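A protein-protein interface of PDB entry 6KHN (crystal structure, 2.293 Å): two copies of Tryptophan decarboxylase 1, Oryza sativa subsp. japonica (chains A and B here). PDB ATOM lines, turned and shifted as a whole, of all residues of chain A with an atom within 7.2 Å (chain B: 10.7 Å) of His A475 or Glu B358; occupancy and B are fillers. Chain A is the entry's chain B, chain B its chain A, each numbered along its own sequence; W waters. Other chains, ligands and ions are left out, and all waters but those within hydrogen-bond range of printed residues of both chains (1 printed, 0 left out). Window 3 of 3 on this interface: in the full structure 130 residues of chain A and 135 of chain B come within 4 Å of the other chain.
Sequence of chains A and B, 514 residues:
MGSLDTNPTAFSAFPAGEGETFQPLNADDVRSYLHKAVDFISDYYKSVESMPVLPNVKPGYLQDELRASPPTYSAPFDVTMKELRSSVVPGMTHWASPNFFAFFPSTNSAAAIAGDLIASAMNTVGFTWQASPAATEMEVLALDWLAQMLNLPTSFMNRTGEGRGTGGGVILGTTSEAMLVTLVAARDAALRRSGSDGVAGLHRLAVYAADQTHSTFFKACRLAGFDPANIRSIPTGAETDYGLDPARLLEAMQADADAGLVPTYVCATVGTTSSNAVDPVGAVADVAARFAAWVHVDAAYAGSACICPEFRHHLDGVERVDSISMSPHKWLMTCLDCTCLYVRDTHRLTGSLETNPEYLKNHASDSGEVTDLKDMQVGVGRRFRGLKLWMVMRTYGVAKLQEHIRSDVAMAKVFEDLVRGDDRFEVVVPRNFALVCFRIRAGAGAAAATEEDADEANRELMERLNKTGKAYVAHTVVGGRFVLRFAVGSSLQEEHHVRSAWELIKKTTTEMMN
Of the 18 printed residues of chain A, 4 touch a printed residue of chain B.
Hydrophobic or aromatic side chains of chain B within 4 Å of the printed part of chain A: Phe B127, Pro B357, Tyr B359 and Leu B360.
Among the printed residues, 9 pairs touch across the chains.
Among the printed residues, no Asp or Glu carboxylate lies within 4 Å of a Lys or Arg side-chain nitrogen of the other chain.
Printed residues of chain B within 4 Å of His A475: Glu B358 (2.9 Å), Tyr B359 (3.4 Å) and Lys B361 (3.99 Å).
Of the printed residues of chain A, Glu B358 touches His A475 (2.9 Å) and Val A477 (3.6 Å).
No residue of chain B comes within 4 Å of Ala A474.
No residue of chain B comes within 4 Å of Thr A476.
Printed residues of chain A within 4 Å of Phe B127: Phe A103 (3.8 Å).
Of the printed residues of chain A, Thr B355 touches Ser A215 (3.9 Å).
Arg A481 touches none of the printed residues of chain B.
The nearest printed residue of chain B that does not touch His A475 is Leu B360 (5.4 Å).
No position is printed for both chains.
The side-chain carboxylate of Glu B358 is in hydrogen-bond range of a ring nitrogen (NE2) of His A475, at 2.9 Å.
The side-chain amide nitrogen of Asn B362 is in hydrogen-bond range of the backbone carbonyl oxygen of Leu B360 (3.1 Å).
The backbone carbonyl oxygen of Phe B127 is in hydrogen-bond range of the backbone NH of Lys B374, at 3.2 Å.
The backbone carbonyl oxygen (O) of Phe A103 sits at hydrogen-bond distance from the guanidinium group (NH1) of Arg A485 (2.7 Å).
NZ of Lys B361 is in salt-bridge range of OE1 of Glu B358 (2.5 Å).
The backbone carbonyl oxygen of Thr B355 sits at hydrogen-bond distance from the side-chain amino group of Lys B374 (2.8 Å).
Phe A103 touches Phe B127.
Tyr B359 touches Phe A103.
Phe A103 touches Leu B360.
OG of Ser A215 touches CB of Thr B355, 3.9 Å away.
Ser A215 touches Pro B357.
CA of Tyr B359 touches O of His A475 (3.4 Å).
CE1 of His A475 touches O of Lys B361, at 3.99 Å.
Val A477 touches Glu B358 (CG2 to CG, 3.6 Å).
Water W1 lies within hydrogen-bond range of O of His A475 (2.7 Å) and O of Tyr B359 (2.9 Å).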
ATOM      1  N   ALA A 102      15.361 -10.727   0.772  1.00  0.00           N
ATOM      2  CA  ALA A 102      14.329 -10.780  -0.254  1.00  0.00           C
ATOM      3  C   ALA A 102      13.630  -9.434  -0.455  1.00  0.00           C
ATOM      4  O   ALA A 102      13.614  -8.562   0.421  1.00  0.00           O
ATOM      5  CB  ALA A 102      13.295 -11.859   0.090  1.00  0.00           C
ATOM      6  N   PHE A 103      13.019  -9.286  -1.628  1.00  0.00           N
ATOM      7  CA  PHE A 103      12.144  -8.136  -1.923  1.00  0.00           C
ATOM      8  C   PHE A 103      12.966  -6.867  -1.704  1.00  0.00           C
ATOM      9  O   PHE A 103      14.066  -6.750  -2.263  1.00  0.00           O
ATOM     10  CB  PHE A 103      10.890  -8.267  -1.073  1.00  0.00           C
ATOM     11  CG  PHE A 103      10.228  -9.607  -1.192  1.00  0.00           C
ATOM     12  CD1 PHE A 103       9.766 -10.055  -2.427  1.00  0.00           C
ATOM     13  CD2 PHE A 103      10.086 -10.431  -0.089  1.00  0.00           C
ATOM     14  CE1 PHE A 103       9.166 -11.300  -2.558  1.00  0.00           C
ATOM     15  CE2 PHE A 103       9.472 -11.678  -0.209  1.00  0.00           C
ATOM     16  CZ  PHE A 103       9.006 -12.110  -1.446  1.00  0.00           C
ATOM     17  N   SER A 215       3.547  -3.765 -11.191  1.00  0.00           N
ATOM     18  CA  SER A 215       2.211  -4.110 -11.658  1.00  0.00           C
ATOM     19  C   SER A 215       1.127  -3.416 -10.850  1.00  0.00           C
ATOM     20  O   SER A 215       0.011  -3.270 -11.346  1.00  0.00           O
ATOM     21  CB  SER A 215       1.990  -5.629 -11.617  1.00  0.00           C
ATOM     22  OG  SER A 215       2.251  -6.135 -10.324  1.00  0.00           O
ATOM     23  N   SER A 274      12.052  -5.219  -9.859  1.00  0.00           N
ATOM     24  CA  SER A 274      12.657  -6.455 -10.338  1.00  0.00           C
ATOM     25  C   SER A 274      14.182  -6.383 -10.324  1.00  0.00           C
ATOM     26  O   SER A 274      14.842  -7.225  -9.702  1.00  0.00           O
ATOM     27  CB  SER A 274      12.150  -6.784 -11.731  1.00  0.00           C
ATOM     28  OG  SER A 274      12.631  -8.054 -12.105  1.00  0.00           O
ATOM     29  N   ASN A 458      18.908 -22.543 -11.054  1.00  0.00           N
ATOM     30  CA  ASN A 458      18.747 -21.375 -10.191  1.00  0.00           C
ATOM     31  C   ASN A 458      17.523 -21.510  -9.289  1.00  0.00           C
ATOM     32  O   ASN A 458      17.560 -21.108  -8.122  1.00  0.00           O
ATOM     33  CB  ASN A 458      18.661 -20.110 -11.040  1.00  0.00           C
ATOM     34  CG  ASN A 458      20.026 -19.635 -11.504  1.00  0.00           C
ATOM     35  OD1 ASN A 458      20.878 -19.286 -10.691  1.00  0.00           O
ATOM     36  ND2 ASN A 458      20.242 -19.632 -12.811  1.00  0.00           N
ATOM     37  N   ARG A 459      16.431 -22.071  -9.803  1.00  0.00           N
ATOM     38  CA  ARG A 459      15.281 -22.327  -8.942  1.00  0.00           C
ATOM     39  C   ARG A 459      15.628 -23.329  -7.847  1.00  0.00           C
ATOM     40  O   ARG A 459      15.243 -23.152  -6.684  1.00  0.00           O
ATOM     41  CB  ARG A 459      14.105 -22.838  -9.770  1.00  0.00           C
ATOM     42  CG  ARG A 459      12.936 -23.310  -8.929  1.00  0.00           C
ATOM     43  CD  ARG A 459      11.663 -23.355  -9.764  1.00  0.00           C
ATOM     44  NE  ARG A 459      10.740 -22.294  -9.367  1.00  0.00           N
ATOM     45  CZ  ARG A 459      10.113 -21.470 -10.205  1.00  0.00           C
ATOM     46  NH1 ARG A 459       9.302 -20.540  -9.717  1.00  0.00           N
ATOM     47  NH2 ARG A 459      10.289 -21.570 -11.522  1.00  0.00           N
ATOM     48  N   MET A 462      17.729 -21.636  -5.150  1.00  0.00           N
ATOM     49  CA  MET A 462      16.938 -20.766  -4.285  1.00  0.00           C
ATOM     50  C   MET A 462      16.156 -21.570  -3.248  1.00  0.00           C
ATOM     51  O   MET A 462      16.091 -21.191  -2.070  1.00  0.00           O
ATOM     52  CB  MET A 462      16.003 -19.912  -5.146  1.00  0.00           C
ATOM     53  CG  MET A 462      14.949 -19.133  -4.366  1.00  0.00           C
ATOM     54  SD  MET A 462      13.727 -18.346  -5.443  1.00  0.00           S
ATOM     55  CE  MET A 462      12.767 -19.763  -5.988  1.00  0.00           C
ATOM     56  N   VAL A 473      15.859 -16.031  -0.007  1.00  0.00           N
ATOM     57  CA  VAL A 473      16.124 -15.500  -1.327  1.00  0.00           C
ATOM     58  C   VAL A 473      14.887 -15.763  -2.175  1.00  0.00           C
ATOM     59  O   VAL A 473      14.231 -16.808  -2.042  1.00  0.00           O
ATOM     60  CB  VAL A 473      17.390 -16.137  -1.926  1.00  0.00           C
ATOM     61  CG1 VAL A 473      17.561 -15.751  -3.360  1.00  0.00           C
ATOM     62  CG2 VAL A 473      18.616 -15.714  -1.106  1.00  0.00           C
ATOM     63  N   ALA A 474      14.521 -14.774  -2.978  1.00  0.00           N
ATOM     64  CA  ALA A 474      13.423 -14.891  -3.915  1.00  0.00           C
ATOM     65  C   ALA A 474      13.908 -14.367  -5.259  1.00  0.00           C
ATOM     66  O   ALA A 474      14.948 -13.713  -5.361  1.00  0.00           O
ATOM     67  CB  ALA A 474      12.175 -14.139  -3.417  1.00  0.00           C
ATOM     68  N   HIS A 475      13.136 -14.653  -6.296  1.00  0.00           N
ATOM     69  CA  HIS A 475      13.609 -14.578  -7.666  1.00  0.00           C
ATOM     70  C   HIS A 475      12.917 -13.463  -8.443  1.00  0.00           C
ATOM     71  O   HIS A 475      11.978 -12.811  -7.974  1.00  0.00           O
ATOM     72  CB  HIS A 475      13.365 -15.910  -8.367  1.00  0.00           C
ATOM     73  CG  HIS A 475      11.940 -16.101  -8.779  1.00  0.00           C
ATOM     74  ND1 HIS A 475      10.949 -16.462  -7.888  1.00  0.00           N
ATOM     75  CD2 HIS A 475      11.330 -15.938  -9.977  1.00  0.00           C
ATOM     76  CE1 HIS A 475       9.795 -16.531  -8.525  1.00  0.00           C
ATOM     77  NE2 HIS A 475       9.998 -16.216  -9.791  1.00  0.00           N
ATOM     78  N   THR A 476      13.392 -13.265  -9.667  1.00  0.00           N
ATOM     79  CA  THR A 476      12.631 -12.527 -10.663  1.00  0.00           C
ATOM     80  C   THR A 476      12.986 -13.070 -12.045  1.00  0.00           C
ATOM     81  O   THR A 476      13.709 -14.056 -12.178  1.00  0.00           O
ATOM     82  CB  THR A 476      12.883 -11.024 -10.536  1.00  0.00           C
ATOM     83  OG1 THR A 476      11.940 -10.326 -11.357  1.00  0.00           O
ATOM     84  CG2 THR A 476      14.292 -10.685 -10.947  1.00  0.00           C
ATOM     85  N   VAL A 477      12.444 -12.445 -13.080  1.00  0.00           N
ATOM     86  CA  VAL A 477      12.747 -12.819 -14.458  1.00  0.00           C
ATOM     87  C   VAL A 477      13.219 -11.567 -15.181  1.00  0.00           C
ATOM     88  O   VAL A 477      12.515 -10.549 -15.198  1.00  0.00           O
ATOM     89  CB  VAL A 477      11.536 -13.445 -15.169  1.00  0.00           C
ATOM     90  CG1 VAL A 477      11.781 -13.493 -16.673  1.00  0.00           C
ATOM     91  CG2 VAL A 477      11.242 -14.846 -14.605  1.00  0.00           C
ATOM     92  N   VAL A 478      14.409 -11.646 -15.767  1.00  0.00           N
ATOM     93  CA  VAL A 478      15.061 -10.528 -16.439  1.00  0.00           C
ATOM     94  C   VAL A 478      15.454 -11.012 -17.824  1.00  0.00           C
ATOM     95  O   VAL A 478      16.229 -11.970 -17.945  1.00  0.00           O
ATOM     96  CB  VAL A 478      16.301 -10.037 -15.671  1.00  0.00           C
ATOM     97  CG1 VAL A 478      17.062  -8.998 -16.478  1.00  0.00           C
ATOM     98  CG2 VAL A 478      15.912  -9.488 -14.312  1.00  0.00           C
ATOM     99  N   ARG A 481      15.094 -14.718 -18.400  1.00  0.00           N
ATOM    100  CA  ARG A 481      15.916 -15.633 -17.623  1.00  0.00           C
ATOM    101  C   ARG A 481      15.520 -15.590 -16.152  1.00  0.00           C
ATOM    102  O   ARG A 481      15.289 -14.513 -15.588  1.00  0.00           O
ATOM    103  CB  ARG A 481      17.396 -15.305 -17.783  1.00  0.00           C
ATOM    104  CG  ARG A 481      17.886 -15.390 -19.222  1.00  0.00           C
ATOM    105  CD  ARG A 481      18.440 -16.768 -19.541  1.00  0.00           C
ATOM    106  NE  ARG A 481      17.417 -17.814 -19.527  1.00  0.00           N
ATOM    107  CZ  ARG A 481      16.616 -18.098 -20.555  1.00  0.00           C
ATOM    108  NH1 ARG A 481      16.721 -17.414 -21.693  1.00  0.00           N
ATOM    109  NH2 ARG A 481      15.706 -19.062 -20.447  1.00  0.00           N
ATOM    110  N   PHE A 482      15.413 -16.778 -15.555  1.00  0.00           N
ATOM    111  CA  PHE A 482      15.203 -16.913 -14.120  1.00  0.00           C
ATOM    112  C   PHE A 482      16.438 -16.402 -13.374  1.00  0.00           C
ATOM    113  O   PHE A 482      17.552 -16.889 -13.594  1.00  0.00           O
ATOM    114  CB  PHE A 482      14.930 -18.377 -13.786  1.00  0.00           C
ATOM    115  CG  PHE A 482      14.492 -18.621 -12.367  1.00  0.00           C
ATOM    116  CD1 PHE A 482      15.416 -18.636 -11.328  1.00  0.00           C
ATOM    117  CD2 PHE A 482      13.156 -18.865 -12.074  1.00  0.00           C
ATOM    118  CE1 PHE A 482      15.006 -18.875 -10.016  1.00  0.00           C
ATOM    119  CE2 PHE A 482      12.743 -19.108 -10.768  1.00  0.00           C
ATOM    120  CZ  PHE A 482      13.667 -19.111  -9.740  1.00  0.00           C
ATOM    121  N   VAL A 483      16.231 -15.447 -12.469  1.00  0.00           N
ATOM    122  CA  VAL A 483      17.298 -14.682 -11.841  1.00  0.00           C
ATOM    123  C   VAL A 483      17.028 -14.601 -10.339  1.00  0.00           C
ATOM    124  O   VAL A 483      15.881 -14.429  -9.915  1.00  0.00           O
ATOM    125  CB  VAL A 483      17.380 -13.278 -12.481  1.00  0.00           C
ATOM    126  CG1 VAL A 483      17.922 -12.253 -11.517  1.00  0.00           C
ATOM    127  CG2 VAL A 483      18.210 -13.332 -13.745  1.00  0.00           C
ATOM    128  N   LEU A 484      18.080 -14.739  -9.532  1.00  0.00           N
ATOM    129  CA  LEU A 484      17.962 -14.574  -8.085  1.00  0.00           C
ATOM    130  C   LEU A 484      18.202 -13.115  -7.718  1.00  0.00           C
ATOM    131  O   LEU A 484      19.122 -12.482  -8.238  1.00  0.00           O
ATOM    132  CB  LEU A 484      18.944 -15.476  -7.328  1.00  0.00           C
ATOM    133  CG  LEU A 484      18.799 -16.981  -7.606  1.00  0.00           C
ATOM    134  CD1 LEU A 484      19.591 -17.834  -6.648  1.00  0.00           C
ATOM    135  CD2 LEU A 484      17.337 -17.384  -7.559  1.00  0.00           C
ATOM    136  N   ARG A 485      17.353 -12.574  -6.858  1.00  0.00           N
ATOM    137  CA  ARG A 485      17.604 -11.256  -6.301  1.00  0.00           C
ATOM    138  C   ARG A 485      18.359 -11.391  -4.988  1.00  0.00           C
ATOM    139  O   ARG A 485      18.222 -12.385  -4.268  1.00  0.00           O
ATOM    140  CB  ARG A 485      16.297 -10.503  -6.068  1.00  0.00           C
ATOM    141  CG  ARG A 485      15.641 -10.000  -7.337  1.00  0.00           C
ATOM    142  CD  ARG A 485      14.258  -9.464  -7.069  1.00  0.00           C
ATOM    143  NE  ARG A 485      14.219  -8.028  -6.781  1.00  0.00           N
ATOM    144  CZ  ARG A 485      14.139  -7.517  -5.555  1.00  0.00           C
ATOM    145  NH1 ARG A 485      14.116  -8.328  -4.503  1.00  0.00           N
ATOM    146  NH2 ARG A 485      14.062  -6.203  -5.376  1.00  0.00           N
ATOM    147  N   PHE B 127       2.255  -9.055   2.117  1.00  0.00           N
ATOM    148  CA  PHE B 127       1.507  -8.963   0.866  1.00  0.00           C
ATOM    149  C   PHE B 127       1.026 -10.332   0.397  1.00  0.00           C
ATOM    150  O   PHE B 127      -0.054 -10.427  -0.179  1.00  0.00           O
ATOM    151  CB  PHE B 127       2.336  -8.282  -0.228  1.00  0.00           C
ATOM    152  CG  PHE B 127       3.822  -8.519  -0.127  1.00  0.00           C
ATOM    153  CD1 PHE B 127       4.373  -9.751  -0.456  1.00  0.00           C
ATOM    154  CD2 PHE B 127       4.665  -7.496   0.235  1.00  0.00           C
ATOM    155  CE1 PHE B 127       5.747  -9.961  -0.402  1.00  0.00           C
ATOM    156  CE2 PHE B 127       6.033  -7.697   0.319  1.00  0.00           C
ATOM    157  CZ  PHE B 127       6.576  -8.938  -0.002  1.00  0.00           C
ATOM    158  N   THR B 128       1.797 -11.395   0.638  1.00  0.00           N
ATOM    159  CA  THR B 128       1.360 -12.761   0.383  1.00  0.00           C
ATOM    160  C   THR B 128       1.353 -13.544   1.688  1.00  0.00           C
ATOM    161  O   THR B 128       2.000 -13.159   2.673  1.00  0.00           O
ATOM    162  CB  THR B 128       2.269 -13.494  -0.622  1.00  0.00           C
ATOM    163  OG1 THR B 128       3.634 -13.458  -0.154  1.00  0.00           O
ATOM    164  CG2 THR B 128       2.176 -12.862  -2.001  1.00  0.00           C
ATOM    165  N   GLN B 130       2.901 -16.321   2.021  1.00  0.00           N
ATOM    166  CA  GLN B 130       4.276 -16.777   2.161  1.00  0.00           C
ATOM    167  C   GLN B 130       5.177 -15.691   2.738  1.00  0.00           C
ATOM    168  O   GLN B 130       6.069 -15.985   3.535  1.00  0.00           O
ATOM    169  CB  GLN B 130       4.817 -17.241   0.806  1.00  0.00           C
ATOM    170  CG  GLN B 130       6.209 -17.909   0.888  1.00  0.00           C
ATOM    171  CD  GLN B 130       6.202 -19.062   1.876  1.00  0.00           C
ATOM    172  OE1 GLN B 130       6.431 -18.869   3.068  1.00  0.00           O
ATOM    173  NE2 GLN B 130       5.898 -20.261   1.392  1.00  0.00           N
ATOM    174  N   THR B 355      -3.174  -9.015  -8.590  1.00  0.00           N
ATOM    175  CA  THR B 355      -2.055  -8.931  -9.507  1.00  0.00           C
ATOM    176  C   THR B 355      -1.297 -10.248  -9.421  1.00  0.00           C
ATOM    177  O   THR B 355      -1.504 -11.044  -8.498  1.00  0.00           O
ATOM    178  CB  THR B 355      -1.143  -7.753  -9.163  1.00  0.00           C
ATOM    179  OG1 THR B 355      -0.704  -7.899  -7.815  1.00  0.00           O
ATOM    180  CG2 THR B 355      -1.901  -6.444  -9.265  1.00  0.00           C
ATOM    181  N   ASN B 356      -0.413 -10.500 -10.379  1.00  0.00           N
ATOM    182  CA  ASN B 356       0.409 -11.708 -10.316  1.00  0.00           C
ATOM    183  C   ASN B 356       1.838 -11.435 -10.770  1.00  0.00           C
ATOM    184  O   ASN B 356       2.375 -12.135 -11.626  1.00  0.00           O
ATOM    185  CB  ASN B 356      -0.241 -12.842 -11.115  1.00  0.00           C
ATOM    186  CG  ASN B 356       0.291 -14.213 -10.707  1.00  0.00           C
ATOM    187  OD1 ASN B 356       0.789 -14.406  -9.579  1.00  0.00           O
ATOM    188  ND2 ASN B 356       0.218 -15.166 -11.627  1.00  0.00           N
ATOM    189  N   PRO B 357       2.508 -10.452 -10.165  1.00  0.00           N
ATOM    190  CA  PRO B 357       3.890 -10.170 -10.560  1.00  0.00           C
ATOM    191  C   PRO B 357       4.809 -11.357 -10.284  1.00  0.00           C
ATOM    192  O   PRO B 357       4.654 -12.081  -9.297  1.00  0.00           O
ATOM    193  CB  PRO B 357       4.265  -8.965  -9.694  1.00  0.00           C
ATOM    194  CG  PRO B 357       3.425  -9.118  -8.487  1.00  0.00           C
ATOM    195  CD  PRO B 357       2.126  -9.688  -8.961  1.00  0.00           C
ATOM    196  N   GLU B 358       5.787 -11.534 -11.179  1.00  0.00           N
ATOM    197  CA  GLU B 358       6.659 -12.700 -11.133  1.00  0.00           C
ATOM    198  C   GLU B 358       7.428 -12.780  -9.817  1.00  0.00           C
ATOM    199  O   GLU B 358       7.554 -13.860  -9.235  1.00  0.00           O
ATOM    200  CB  GLU B 358       7.630 -12.660 -12.312  1.00  0.00           C
ATOM    201  CG  GLU B 358       8.598 -13.839 -12.353  1.00  0.00           C
ATOM    202  CD  GLU B 358       7.891 -15.148 -12.652  1.00  0.00           C
ATOM    203  OE1 GLU B 358       6.905 -15.131 -13.428  1.00  0.00           O
ATOM    204  OE2 GLU B 358       8.314 -16.194 -12.111  1.00  0.00           O
ATOM    205  N   TYR B 359       7.923 -11.643  -9.317  1.00  0.00           N
ATOM    206  CA  TYR B 359       8.799 -11.676  -8.151  1.00  0.00           C
ATOM    207  C   TYR B 359       8.065 -12.087  -6.876  1.00  0.00           C
ATOM    208  O   TYR B 359       8.725 -12.483  -5.903  1.00  0.00           O
ATOM    209  CB  TYR B 359       9.492 -10.319  -7.974  1.00  0.00           C
ATOM    210  CG  TYR B 359       8.667  -9.285  -7.244  1.00  0.00           C
ATOM    211  CD1 TYR B 359       7.586  -8.654  -7.866  1.00  0.00           C
ATOM    212  CD2 TYR B 359       8.973  -8.927  -5.934  1.00  0.00           C
ATOM    213  CE1 TYR B 359       6.828  -7.706  -7.205  1.00  0.00           C
ATOM    214  CE2 TYR B 359       8.222  -7.973  -5.259  1.00  0.00           C
ATOM    215  CZ  TYR B 359       7.143  -7.372  -5.895  1.00  0.00           C
ATOM    216  OH  TYR B 359       6.398  -6.426  -5.216  1.00  0.00           O
ATOM    217  N   LEU B 360       6.726 -12.056  -6.876  1.00  0.00           N
ATOM    218  CA  LEU B 360       5.919 -12.484  -5.739  1.00  0.00           C
ATOM    219  C   LEU B 360       5.463 -13.938  -5.824  1.00  0.00           C
ATOM    220  O   LEU B 360       4.869 -14.439  -4.860  1.00  0.00           O
ATOM    221  CB  LEU B 360       4.693 -11.581  -5.588  1.00  0.00           C
ATOM    222  CG  LEU B 360       5.072 -10.185  -5.083  1.00  0.00           C
ATOM    223  CD1 LEU B 360       3.844  -9.406  -4.672  1.00  0.00           C
ATOM    224  CD2 LEU B 360       6.066 -10.302  -3.903  1.00  0.00           C
ATOM    225  N   LYS B 361       5.742 -14.639  -6.920  1.00  0.00           N
ATOM    226  CA  LYS B 361       5.176 -15.973  -7.102  1.00  0.00           C
ATOM    227  C   LYS B 361       5.747 -16.956  -6.088  1.00  0.00           C
ATOM    228  O   LYS B 361       6.940 -16.914  -5.767  1.00  0.00           O
ATOM    229  CB  LYS B 361       5.428 -16.480  -8.521  1.00  0.00           C
ATOM    230  CG  LYS B 361       4.396 -15.966  -9.513  1.00  0.00           C
ATOM    231  CD  LYS B 361       4.849 -16.150 -10.946  1.00  0.00           C
ATOM    232  CE  LYS B 361       3.812 -15.607 -11.939  1.00  0.00           C
ATOM    233  NZ  LYS B 361       4.425 -15.530 -13.300  1.00  0.00           N
ATOM    234  N   ASN B 362       4.883 -17.843  -5.589  1.00  0.00           N
ATOM    235  CA  ASN B 362       5.286 -18.875  -4.641  1.00  0.00           C
ATOM    236  C   ASN B 362       4.312 -20.035  -4.751  1.00  0.00           C
ATOM    237  O   ASN B 362       3.230 -19.901  -5.323  1.00  0.00           O
ATOM    238  CB  ASN B 362       5.320 -18.346  -3.198  1.00  0.00           C
ATOM    239  CG  ASN B 362       3.959 -17.863  -2.733  1.00  0.00           C
ATOM    240  OD1 ASN B 362       3.215 -18.592  -2.071  1.00  0.00           O
ATOM    241  ND2 ASN B 362       3.616 -16.635  -3.098  1.00  0.00           N
ATOM    242  N   HIS B 363       4.692 -21.174  -4.166  1.00  0.00           N
ATOM    243  CA  HIS B 363       3.896 -22.394  -4.332  1.00  0.00           C
ATOM    244  C   HIS B 363       2.569 -22.311  -3.587  1.00  0.00           C
ATOM    245  O   HIS B 363       1.548 -22.817  -4.073  1.00  0.00           O
ATOM    246  CB  HIS B 363       4.685 -23.623  -3.878  1.00  0.00           C
ATOM    247  CG  HIS B 363       5.927 -23.879  -4.681  1.00  0.00           C
ATOM    248  ND1 HIS B 363       5.923 -23.955  -6.061  1.00  0.00           N
ATOM    249  CD2 HIS B 363       7.215 -24.074  -4.298  1.00  0.00           C
ATOM    250  CE1 HIS B 363       7.153 -24.187  -6.490  1.00  0.00           C
ATOM    251  NE2 HIS B 363       7.955 -24.266  -5.440  1.00  0.00           N
ATOM    252  N   SER B 365       0.655 -19.670  -3.061  1.00  0.00           N
ATOM    253  CA  SER B 365      -0.284 -18.878  -3.842  1.00  0.00           C
ATOM    254  C   SER B 365      -0.778 -19.653  -5.060  1.00  0.00           C
ATOM    255  O   SER B 365      -1.970 -19.630  -5.368  1.00  0.00           O
ATOM    256  CB  SER B 365       0.374 -17.571  -4.275  1.00  0.00           C
ATOM    257  OG  SER B 365       0.599 -16.738  -3.163  1.00  0.00           O
ATOM    258  N   ASP B 366       0.133 -20.340  -5.761  1.00  0.00           N
ATOM    259  CA  ASP B 366      -0.246 -21.162  -6.908  1.00  0.00           C
ATOM    260  C   ASP B 366      -1.268 -22.227  -6.536  1.00  0.00           C
ATOM    261  O   ASP B 366      -2.113 -22.587  -7.361  1.00  0.00           O
ATOM    262  CB  ASP B 366       0.986 -21.847  -7.502  1.00  0.00           C
ATOM    263  CG  ASP B 366       1.931 -20.881  -8.179  1.00  0.00           C
ATOM    264  OD1 ASP B 366       1.549 -19.705  -8.375  1.00  0.00           O
ATOM    265  OD2 ASP B 366       3.068 -21.300  -8.504  1.00  0.00           O
ATOM    266  N   LYS B 374      -2.801  -8.803  -0.383  1.00  0.00           N
ATOM    267  CA  LYS B 374      -2.632  -7.768  -1.399  1.00  0.00           C
ATOM    268  C   LYS B 374      -3.754  -7.786  -2.440  1.00  0.00           C
ATOM    269  O   LYS B 374      -4.034  -6.748  -3.047  1.00  0.00           O
ATOM    270  CB  LYS B 374      -1.286  -7.920  -2.100  1.00  0.00           C
ATOM    271  CG  LYS B 374      -1.164  -9.184  -2.940  1.00  0.00           C
ATOM    272  CD  LYS B 374       0.024  -9.080  -3.872  1.00  0.00           C
ATOM    273  CE  LYS B 374       0.179 -10.335  -4.713  1.00  0.00           C
ATOM    274  NZ  LYS B 374      -0.694 -10.244  -5.910  1.00  0.00           N
ATOM    275  N   VAL B 380       0.161  -3.023  -2.128  1.00  0.00           N
ATOM    276  CA  VAL B 380       0.866  -4.298  -2.081  1.00  0.00           C
ATOM    277  C   VAL B 380       1.241  -4.619  -0.640  1.00  0.00           C
ATOM    278  O   VAL B 380       0.746  -5.595  -0.063  1.00  0.00           O
ATOM    279  CB  VAL B 380       2.113  -4.281  -2.978  1.00  0.00           C
ATOM    280  CG1 VAL B 380       2.746  -5.681  -3.037  1.00  0.00           C
ATOM    281  CG2 VAL B 380       1.753  -3.745  -4.359  1.00  0.00           C
HETATM  282  O   HOH W   1      11.502 -11.708  -5.519  1.00  0.00           O
